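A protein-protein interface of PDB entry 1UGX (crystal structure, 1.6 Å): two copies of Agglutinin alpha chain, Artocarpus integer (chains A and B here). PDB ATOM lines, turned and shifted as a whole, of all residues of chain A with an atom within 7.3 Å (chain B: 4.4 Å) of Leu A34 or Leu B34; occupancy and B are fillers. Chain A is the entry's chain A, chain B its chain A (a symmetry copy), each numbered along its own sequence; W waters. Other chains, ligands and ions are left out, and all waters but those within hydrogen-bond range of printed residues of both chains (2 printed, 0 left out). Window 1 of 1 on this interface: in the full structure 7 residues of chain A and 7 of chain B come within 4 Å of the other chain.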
ATOM      1  N   ASP A   6      32.370   5.079   4.705  1.00  0.00           N
ATOM      2  CA  ASP A   6      32.181   4.009   3.723  1.00  0.00           C
ATOM      3  C   ASP A   6      31.758   4.552   2.370  1.00  0.00           C
ATOM      4  O   ASP A   6      32.063   3.967   1.337  1.00  0.00           O
ATOM      5  CB  ASP A   6      31.124   3.004   4.184  1.00  0.00           C
ATOM      6  CG  ASP A   6      31.582   2.156   5.354  1.00  0.00           C
ATOM      7  OD1 ASP A   6      32.797   2.114   5.628  1.00  0.00           O
ATOM      8  OD2 ASP A   6      30.714   1.523   5.982  1.00  0.00           O
ATOM      9  N   GLY A   7      31.056   5.676   2.379  1.00  0.00           N
ATOM     10  CA  GLY A   7      30.590   6.240   1.124  1.00  0.00           C
ATOM     11  C   GLY A   7      29.185   5.757   0.813  1.00  0.00           C
ATOM     12  O   GLY A   7      28.511   5.169   1.666  1.00  0.00           O
ATOM     13  N   ALA A   8      28.740   5.990  -0.420  1.00  0.00           N
ATOM     14  CA  ALA A   8      27.399   5.599  -0.833  1.00  0.00           C
ATOM     15  C   ALA A   8      27.376   4.377  -1.746  1.00  0.00           C
ATOM     16  O   ALA A   8      28.262   4.200  -2.598  1.00  0.00           O
ATOM     17  CB  ALA A   8      26.714   6.778  -1.527  1.00  0.00           C
ATOM     18  N   PHE A   9      26.354   3.545  -1.561  1.00  0.00           N
ATOM     19  CA  PHE A   9      26.172   2.327  -2.340  1.00  0.00           C
ATOM     20  C   PHE A   9      24.744   2.235  -2.865  1.00  0.00           C
ATOM     21  O   PHE A   9      24.038   3.246  -2.913  1.00  0.00           O
ATOM     22  CB  PHE A   9      26.515   1.103  -1.484  1.00  0.00           C
ATOM     23  CG  PHE A   9      27.948   1.078  -1.036  1.00  0.00           C
ATOM     24  CD1 PHE A   9      28.370   1.857   0.033  1.00  0.00           C
ATOM     25  CD2 PHE A   9      28.890   0.326  -1.731  1.00  0.00           C
ATOM     26  CE1 PHE A   9      29.712   1.897   0.404  1.00  0.00           C
ATOM     27  CE2 PHE A   9      30.235   0.359  -1.369  1.00  0.00           C
ATOM     28  CZ  PHE A   9      30.645   1.147  -0.299  1.00  0.00           C
ATOM     29  N   THR A  10      24.322   1.031  -3.251  1.00  0.00           N
ATOM     30  CA  THR A  10      22.988   0.810  -3.815  1.00  0.00           C
ATOM     31  C   THR A  10      21.946   0.375  -2.788  1.00  0.00           C
ATOM     32  O   THR A  10      20.745   0.455  -3.037  1.00  0.00           O
ATOM     33  CB  THR A  10      23.020  -0.283  -4.919  1.00  0.00           C
ATOM     34  OG1 THR A  10      24.207  -0.148  -5.704  1.00  0.00           O
ATOM     35  CG2 THR A  10      21.808  -0.143  -5.834  1.00  0.00           C
ATOM     36  N   GLY A  11      22.407  -0.102  -1.639  1.00  0.00           N
ATOM     37  CA  GLY A  11      21.484  -0.546  -0.616  1.00  0.00           C
ATOM     38  C   GLY A  11      22.259  -1.200   0.507  1.00  0.00           C
ATOM     39  O   GLY A  11      23.487  -1.149   0.517  1.00  0.00           O
ATOM     40  N   ILE A  12      21.544  -1.801   1.447  1.00  0.00           N
ATOM     41  CA  ILE A  12      22.172  -2.464   2.586  1.00  0.00           C
ATOM     42  C   ILE A  12      21.689  -3.902   2.686  1.00  0.00           C
ATOM     43  O   ILE A  12      20.493  -4.174   2.612  1.00  0.00           O
ATOM     44  CB  ILE A  12      21.837  -1.726   3.894  1.00  0.00           C
ATOM     45  CG1 ILE A  12      22.413  -0.308   3.850  1.00  0.00           C
ATOM     46  CG2 ILE A  12      22.407  -2.487   5.091  1.00  0.00           C
ATOM     47  CD1 ILE A  12      22.030   0.533   5.043  1.00  0.00           C
ATOM     48  N   ARG A  13      22.631  -4.826   2.853  1.00  0.00           N
ATOM     49  CA  ARG A  13      22.293  -6.238   2.957  1.00  0.00           C
ATOM     50  C   ARG A  13      22.457  -6.771   4.372  1.00  0.00           C
ATOM     51  O   ARG A  13      21.647  -7.575   4.829  1.00  0.00           O
ATOM     52  CB  ARG A  13      23.167  -7.059   2.007  1.00  0.00           C
ATOM     53  CG  ARG A  13      22.796  -6.923   0.536  1.00  0.00           C
ATOM     54  CD  ARG A  13      23.900  -7.486  -0.350  1.00  0.00           C
ATOM     55  NE  ARG A  13      23.514  -7.529  -1.758  1.00  0.00           N
ATOM     56  CZ  ARG A  13      22.869  -8.541  -2.330  1.00  0.00           C
ATOM     57  NH1 ARG A  13      22.559  -8.486  -3.617  1.00  0.00           N
ATOM     58  NH2 ARG A  13      22.546  -9.616  -1.623  1.00  0.00           N
ATOM     59  N   VAL A  31      27.620  -4.745   5.158  1.00  0.00           N
ATOM     60  CA  VAL A  31      27.746  -5.425   3.878  1.00  0.00           C
ATOM     61  C   VAL A  31      26.705  -4.702   3.035  1.00  0.00           C
ATOM     62  O   VAL A  31      25.502  -4.797   3.294  1.00  0.00           O
ATOM     63  CB  VAL A  31      27.396  -6.921   3.949  1.00  0.00           C
ATOM     64  CG1 VAL A  31      27.484  -7.535   2.550  1.00  0.00           C
ATOM     65  CG2 VAL A  31      28.365  -7.631   4.886  1.00  0.00           C
ATOM     66  N   TYR A  32      27.179  -3.950   2.055  1.00  0.00           N
ATOM     67  CA  TYR A  32      26.291  -3.186   1.190  1.00  0.00           C
ATOM     68  C   TYR A  32      25.936  -3.936  -0.068  1.00  0.00           C
ATOM     69  O   TYR A  32      26.496  -4.992  -0.369  1.00  0.00           O
ATOM     70  CB  TYR A  32      26.959  -1.881   0.749  1.00  0.00           C
ATOM     71  CG  TYR A  32      27.326  -0.937   1.857  1.00  0.00           C
ATOM     72  CD1 TYR A  32      28.597  -0.962   2.440  1.00  0.00           C
ATOM     73  CD2 TYR A  32      26.398  -0.012   2.332  1.00  0.00           C
ATOM     74  CE1 TYR A  32      28.931  -0.081   3.466  1.00  0.00           C
ATOM     75  CE2 TYR A  32      26.718   0.863   3.354  1.00  0.00           C
ATOM     76  CZ  TYR A  32      27.984   0.826   3.918  1.00  0.00           C
ATOM     77  OH  TYR A  32      28.291   1.699   4.931  1.00  0.00           O
ATOM     78  N   ASP A  33      24.975  -3.388  -0.800  1.00  0.00           N
ATOM     79  CA  ASP A  33      24.640  -3.952  -2.087  1.00  0.00           C
ATOM     80  C   ASP A  33      25.306  -2.980  -3.034  1.00  0.00           C
ATOM     81  O   ASP A  33      25.277  -1.770  -2.804  1.00  0.00           O
ATOM     82  CB  ASP A  33      23.149  -3.927  -2.392  1.00  0.00           C
ATOM     83  CG  ASP A  33      22.857  -4.443  -3.787  1.00  0.00           C
ATOM     84  OD1 ASP A  33      23.028  -5.659  -4.007  1.00  0.00           O
ATOM     85  OD2 ASP A  33      22.486  -3.636  -4.672  1.00  0.00           O
ATOM     86  N   LEU A  34      25.933  -3.503  -4.078  1.00  0.00           N
ATOM     87  CA  LEU A  34      26.562  -2.655  -5.073  1.00  0.00           C
ATOM     88  C   LEU A  34      26.055  -3.147  -6.415  1.00  0.00           C
ATOM     89  O   LEU A  34      26.584  -4.101  -6.982  1.00  0.00           O
ATOM     90  CB  LEU A  34      28.087  -2.759  -5.018  1.00  0.00           C
ATOM     91  CG  LEU A  34      28.840  -1.934  -6.071  1.00  0.00           C
ATOM     92  CD1 LEU A  34      28.515  -0.449  -5.913  1.00  0.00           C
ATOM     93  CD2 LEU A  34      30.334  -2.170  -5.923  1.00  0.00           C
ATOM     94  N   ASN A  35      24.995  -2.507  -6.895  1.00  0.00           N
ATOM     95  CA  ASN A  35      24.409  -2.855  -8.174  1.00  0.00           C
ATOM     96  C   ASN A  35      24.068  -4.334  -8.321  1.00  0.00           C
ATOM     97  O   ASN A  35      24.371  -4.952  -9.345  1.00  0.00           O
ATOM     98  CB  ASN A  35      25.351  -2.399  -9.291  1.00  0.00           C
ATOM     99  CG  ASN A  35      25.622  -0.909  -9.232  1.00  0.00           C
ATOM    100  OD1 ASN A  35      26.770  -0.462  -9.267  1.00  0.00           O
ATOM    101  ND2 ASN A  35      24.558  -0.129  -9.127  1.00  0.00           N
ATOM    102  N   GLY A  36      23.445  -4.900  -7.290  1.00  0.00           N
ATOM    103  CA  GLY A  36      23.038  -6.293  -7.349  1.00  0.00           C
ATOM    104  C   GLY A  36      23.960  -7.321  -6.733  1.00  0.00           C
ATOM    105  O   GLY A  36      23.584  -8.486  -6.619  1.00  0.00           O
ATOM    106  N   SER A  37      25.162  -6.910  -6.348  1.00  0.00           N
ATOM    107  CA  SER A  37      26.115  -7.828  -5.742  1.00  0.00           C
ATOM    108  C   SER A  37      26.526  -7.334  -4.368  1.00  0.00           C
ATOM    109  O   SER A  37      26.549  -6.134  -4.104  1.00  0.00           O
ATOM    110  CB  SER A  37      27.357  -7.976  -6.621  1.00  0.00           C
ATOM    111  OG  SER A  37      27.028  -8.555  -7.874  1.00  0.00           O
ATOM    112  N   PRO A  38      26.852  -8.263  -3.466  1.00  0.00           N
ATOM    113  CA  PRO A  38      27.257  -7.843  -2.125  1.00  0.00           C
ATOM    114  C   PRO A  38      28.618  -7.165  -2.166  1.00  0.00           C
ATOM    115  O   PRO A  38      29.488  -7.538  -2.956  1.00  0.00           O
ATOM    116  CB  PRO A  38      27.314  -9.159  -1.345  1.00  0.00           C
ATOM    117  CG  PRO A  38      26.419 -10.082  -2.120  1.00  0.00           C
ATOM    118  CD  PRO A  38      26.726  -9.728  -3.545  1.00  0.00           C
ATOM    119  N   TYR A  39      28.794  -6.153  -1.328  1.00  0.00           N
ATOM    120  CA  TYR A  39      30.072  -5.471  -1.232  1.00  0.00           C
ATOM    121  C   TYR A  39      30.374  -5.357   0.251  1.00  0.00           C
ATOM    122  O   TYR A  39      29.683  -4.651   0.983  1.00  0.00           O
ATOM    123  CB  TYR A  39      30.021  -4.086  -1.880  1.00  0.00           C
ATOM    124  CG  TYR A  39      31.340  -3.360  -1.790  1.00  0.00           C
ATOM    125  CD1 TYR A  39      31.682  -2.640  -0.647  1.00  0.00           C
ATOM    126  CD2 TYR A  39      32.271  -3.431  -2.827  1.00  0.00           C
ATOM    127  CE1 TYR A  39      32.917  -2.011  -0.533  1.00  0.00           C
ATOM    128  CE2 TYR A  39      33.514  -2.804  -2.723  1.00  0.00           C
ATOM    129  CZ  TYR A  39      33.827  -2.096  -1.571  1.00  0.00           C
ATOM    130  OH  TYR A  39      35.048  -1.474  -1.449  1.00  0.00           O
ATOM    131  N   PHE A  60      17.245  -8.520   1.661  1.00  0.00           N
ATOM    132  CA  PHE A  60      17.409  -7.609   0.533  1.00  0.00           C
ATOM    133  C   PHE A  60      16.898  -8.277  -0.744  1.00  0.00           C
ATOM    134  O   PHE A  60      17.151  -9.460  -0.968  1.00  0.00           O
ATOM    135  CB  PHE A  60      18.893  -7.273   0.371  1.00  0.00           C
ATOM    136  CG  PHE A  60      19.185  -6.318  -0.746  1.00  0.00           C
ATOM    137  CD1 PHE A  60      19.029  -4.949  -0.568  1.00  0.00           C
ATOM    138  CD2 PHE A  60      19.621  -6.788  -1.981  1.00  0.00           C
ATOM    139  CE1 PHE A  60      19.304  -4.059  -1.603  1.00  0.00           C
ATOM    140  CE2 PHE A  60      19.901  -5.906  -3.024  1.00  0.00           C
ATOM    141  CZ  PHE A  60      19.742  -4.541  -2.836  1.00  0.00           C
ATOM    142  N   PHE B   9      27.958   4.245 -10.005  1.00  0.00           N
ATOM    143  CA  PHE B   9      29.117   4.374  -9.131  1.00  0.00           C
ATOM    144  C   PHE B   9      29.324   5.827  -8.725  1.00  0.00           C
ATOM    145  O   PHE B   9      28.399   6.637  -8.835  1.00  0.00           O
ATOM    146  CB  PHE B   9      30.363   3.823  -9.832  1.00  0.00           C
ATOM    147  CG  PHE B   9      30.265   2.358 -10.150  1.00  0.00           C
ATOM    148  CD1 PHE B   9      29.538   1.920 -11.249  1.00  0.00           C
ATOM    149  CD2 PHE B   9      30.842   1.414  -9.307  1.00  0.00           C
ATOM    150  CE1 PHE B   9      29.378   0.560 -11.505  1.00  0.00           C
ATOM    151  CE2 PHE B   9      30.688   0.052  -9.554  1.00  0.00           C
ATOM    152  CZ  PHE B   9      29.954  -0.375 -10.655  1.00  0.00           C
ATOM    153  N   THR B  10      30.531   6.156  -8.262  1.00  0.00           N
ATOM    154  CA  THR B  10      30.852   7.507  -7.797  1.00  0.00           C
ATOM    155  C   THR B  10      31.489   8.395  -8.863  1.00  0.00           C
ATOM    156  O   THR B  10      31.525   9.616  -8.727  1.00  0.00           O
ATOM    157  CB  THR B  10      31.835   7.467  -6.594  1.00  0.00           C
ATOM    158  OG1 THR B  10      31.500   6.383  -5.726  1.00  0.00           O
ATOM    159  CG2 THR B  10      31.756   8.769  -5.805  1.00  0.00           C
ATOM    160  N   TYR B  32      35.595   2.295 -12.798  1.00  0.00           N
ATOM    161  CA  TYR B  32      34.865   3.337 -12.090  1.00  0.00           C
ATOM    162  C   TYR B  32      35.539   3.731 -10.801  1.00  0.00           C
ATOM    163  O   TYR B  32      36.494   3.094 -10.353  1.00  0.00           O
ATOM    164  CB  TYR B  32      33.460   2.855 -11.721  1.00  0.00           C
ATOM    165  CG  TYR B  32      32.579   2.484 -12.879  1.00  0.00           C
ATOM    166  CD1 TYR B  32      32.510   1.168 -13.345  1.00  0.00           C
ATOM    167  CD2 TYR B  32      31.809   3.454 -13.519  1.00  0.00           C
ATOM    168  CE1 TYR B  32      31.689   0.830 -14.418  1.00  0.00           C
ATOM    169  CE2 TYR B  32      30.996   3.131 -14.589  1.00  0.00           C
ATOM    170  CZ  TYR B  32      30.937   1.819 -15.035  1.00  0.00           C
ATOM    171  OH  TYR B  32      30.125   1.510 -16.098  1.00  0.00           O
ATOM    172  N   ASP B  33      35.042   4.810 -10.211  1.00  0.00           N
ATOM    173  CA  ASP B  33      35.528   5.206  -8.909  1.00  0.00           C
ATOM    174  C   ASP B  33      34.408   4.740  -8.006  1.00  0.00           C
ATOM    175  O   ASP B  33      33.234   4.874  -8.353  1.00  0.00           O
ATOM    176  CB  ASP B  33      35.646   6.714  -8.738  1.00  0.00           C
ATOM    177  CG  ASP B  33      36.069   7.084  -7.330  1.00  0.00           C
ATOM    178  OD1 ASP B  33      37.234   6.807  -6.980  1.00  0.00           O
ATOM    179  OD2 ASP B  33      35.236   7.621  -6.562  1.00  0.00           O
ATOM    180  N   LEU B  34      34.765   4.166  -6.867  1.00  0.00           N
ATOM    181  CA  LEU B  34      33.768   3.728  -5.907  1.00  0.00           C
ATOM    182  C   LEU B  34      34.197   4.307  -4.573  1.00  0.00           C
ATOM    183  O   LEU B  34      35.033   3.738  -3.874  1.00  0.00           O
ATOM    184  CB  LEU B  34      33.703   2.202  -5.820  1.00  0.00           C
ATOM    185  CG  LEU B  34      32.710   1.645  -4.791  1.00  0.00           C
ATOM    186  CD1 LEU B  34      31.291   2.107  -5.118  1.00  0.00           C
ATOM    187  CD2 LEU B  34      32.787   0.127  -4.786  1.00  0.00           C
ATOM    188  N   ASN B  35      33.642   5.469  -4.250  1.00  0.00           N
ATOM    189  CA  ASN B  35      33.943   6.137  -2.999  1.00  0.00           C
ATOM    190  C   ASN B  35      35.432   6.332  -2.740  1.00  0.00           C
ATOM    191  O   ASN B  35      35.922   6.066  -1.639  1.00  0.00           O
ATOM    192  CB  ASN B  35      33.288   5.359  -1.854  1.00  0.00           C
ATOM    193  CG  ASN B  35      31.788   5.242  -2.033  1.00  0.00           C
ATOM    194  OD1 ASN B  35      31.212   4.156  -1.941  1.00  0.00           O
ATOM    195  ND2 ASN B  35      31.146   6.367  -2.304  1.00  0.00           N
ATOM    196  N   GLY B  36      36.153   6.791  -3.762  1.00  0.00           N
ATOM    197  CA  GLY B  36      37.572   7.053  -3.604  1.00  0.00           C
ATOM    198  C   GLY B  36      38.538   5.974  -4.036  1.00  0.00           C
ATOM    199  O   GLY B  36      39.744   6.212  -4.070  1.00  0.00           O
ATOM    200  N   SER B  37      38.028   4.789  -4.354  1.00  0.00           N
ATOM    201  CA  SER B  37      38.881   3.692  -4.784  1.00  0.00           C
ATOM    202  C   SER B  37      38.465   3.204  -6.159  1.00  0.00           C
ATOM    203  O   SER B  37      37.296   3.282  -6.535  1.00  0.00           O
ATOM    204  CB  SER B  37      38.811   2.531  -3.791  1.00  0.00           C
ATOM    205  OG  SER B  37      39.313   2.917  -2.522  1.00  0.00           O
ATOM    206  N   TYR B  39      37.301   0.791  -9.091  1.00  0.00           N
ATOM    207  CA  TYR B  39      36.489  -0.412  -9.142  1.00  0.00           C
ATOM    208  C   TYR B  39      36.470  -0.842 -10.598  1.00  0.00           C
ATOM    209  O   TYR B  39      35.913  -0.154 -11.450  1.00  0.00           O
ATOM    210  CB  TYR B  39      35.068  -0.154  -8.637  1.00  0.00           C
ATOM    211  CG  TYR B  39      34.207  -1.392  -8.682  1.00  0.00           C
ATOM    212  CD1 TYR B  39      33.555  -1.765  -9.856  1.00  0.00           C
ATOM    213  CD2 TYR B  39      34.083  -2.221  -7.567  1.00  0.00           C
ATOM    214  CE1 TYR B  39      32.803  -2.932  -9.923  1.00  0.00           C
ATOM    215  CE2 TYR B  39      33.330  -3.396  -7.624  1.00  0.00           C
ATOM    216  CZ  TYR B  39      32.694  -3.742  -8.807  1.00  0.00           C
ATOM    217  OH  TYR B  39      31.950  -4.897  -8.882  1.00  0.00           O
HETATM  218  O   HOH W   1      34.496   1.723  -1.517  1.00  0.00           O
HETATM  219  O   HOH W   2      28.842  -4.009  -9.171  1.00  0.00           O
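The backbone carbonyl oxygen of Ala A8 lies close to the side-chain amide oxygen of Asn B35 (3.0 Å).
O of Asp A6 lies close to OD1 of Asn B35 (3.4 Å).
The side-chain hydroxyl (OG1) of Thr A10 is in hydrogen-bond range of the backbone NH (N) of Asn A35, at 2.8 Å.
The side-chain hydroxyl of Thr B10 sits at hydrogen-bond distance from the backbone NH of Asn B35 (2.8 Å).
The side-chain hydroxyl (OH) of Tyr A32 lies within hydrogen-bond range of the side-chain carboxylate (OD2) of Asp A6 (2.6 Å).
The backbone NH (N) of Tyr B39 is in hydrogen-bond range of the backbone carbonyl oxygen (O) of Tyr B32.
N of Tyr A39 is in hydrogen-bond range of O of Tyr A32 (2.7 Å).
Among the printed residues, merely in contact across the chains: Phe A9 with Asn B35 (3.5 Å), Asn A35 with Phe B9 (3.5 Å), Gly A7 with Asn B35 (3.5 Å), Leu A34 with Leu B34 (3.5 Å), Leu A34 with Tyr B39 (3.7 Å) and Tyr A39 with Leu B34 (3.7 Å).
Leu A34 touches just these residues of chain B: Leu B34 and Tyr B39.
Of the printed residues of chain A, Leu B34 touches Leu A34 (3.5 Å) and Tyr A39 (3.7 Å).
Printed residues of chain B within 4 Å of Asn A35: Phe B9.
Printed residues of chain B within 4 Å of Ala A8: Asn B35 (3.0 Å).
Of the printed residues of chain A, Asn B35 touches Asp A6, Gly A7, Ala A8 and Phe A9.
Ser B37 touches none of the printed residues of chain A.
The nearest residue of chain A that does not touch Leu B34 is Phe A9 (4.3 Å).
The nearest printed residue of chain B that does not touch Phe A9 is Leu B34 (4.3 Å).
Of the 18 printed residues of chain A, 7 touch a printed residue of chain B.
Along chain A the printed residues that touch a printed residue of chain B span positions 6 to 39.
Of the 9 printed residues of chain B, 4 touch a printed residue of chain A.
Printed residues of chain B that touch a printed residue of chain A: Phe B9, Leu B34, Asn B35 and Tyr B39.
Phe A9 touches Asn B35, and with the chains exchanged Asn A35 touches Phe B9.
Leu A34 touches its own counterpart, Leu B34.
Leu A34 touches Tyr B39, and with the chains exchanged Tyr A39 touches Leu B34.
Water W2 bridges the backbone carbonyl oxygen of Leu A34 (3.1 Å) and the side-chain hydroxyl of Tyr B39 (3.2 Å).
Water W1 bridges O of Leu B34 and OH of Tyr A39.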
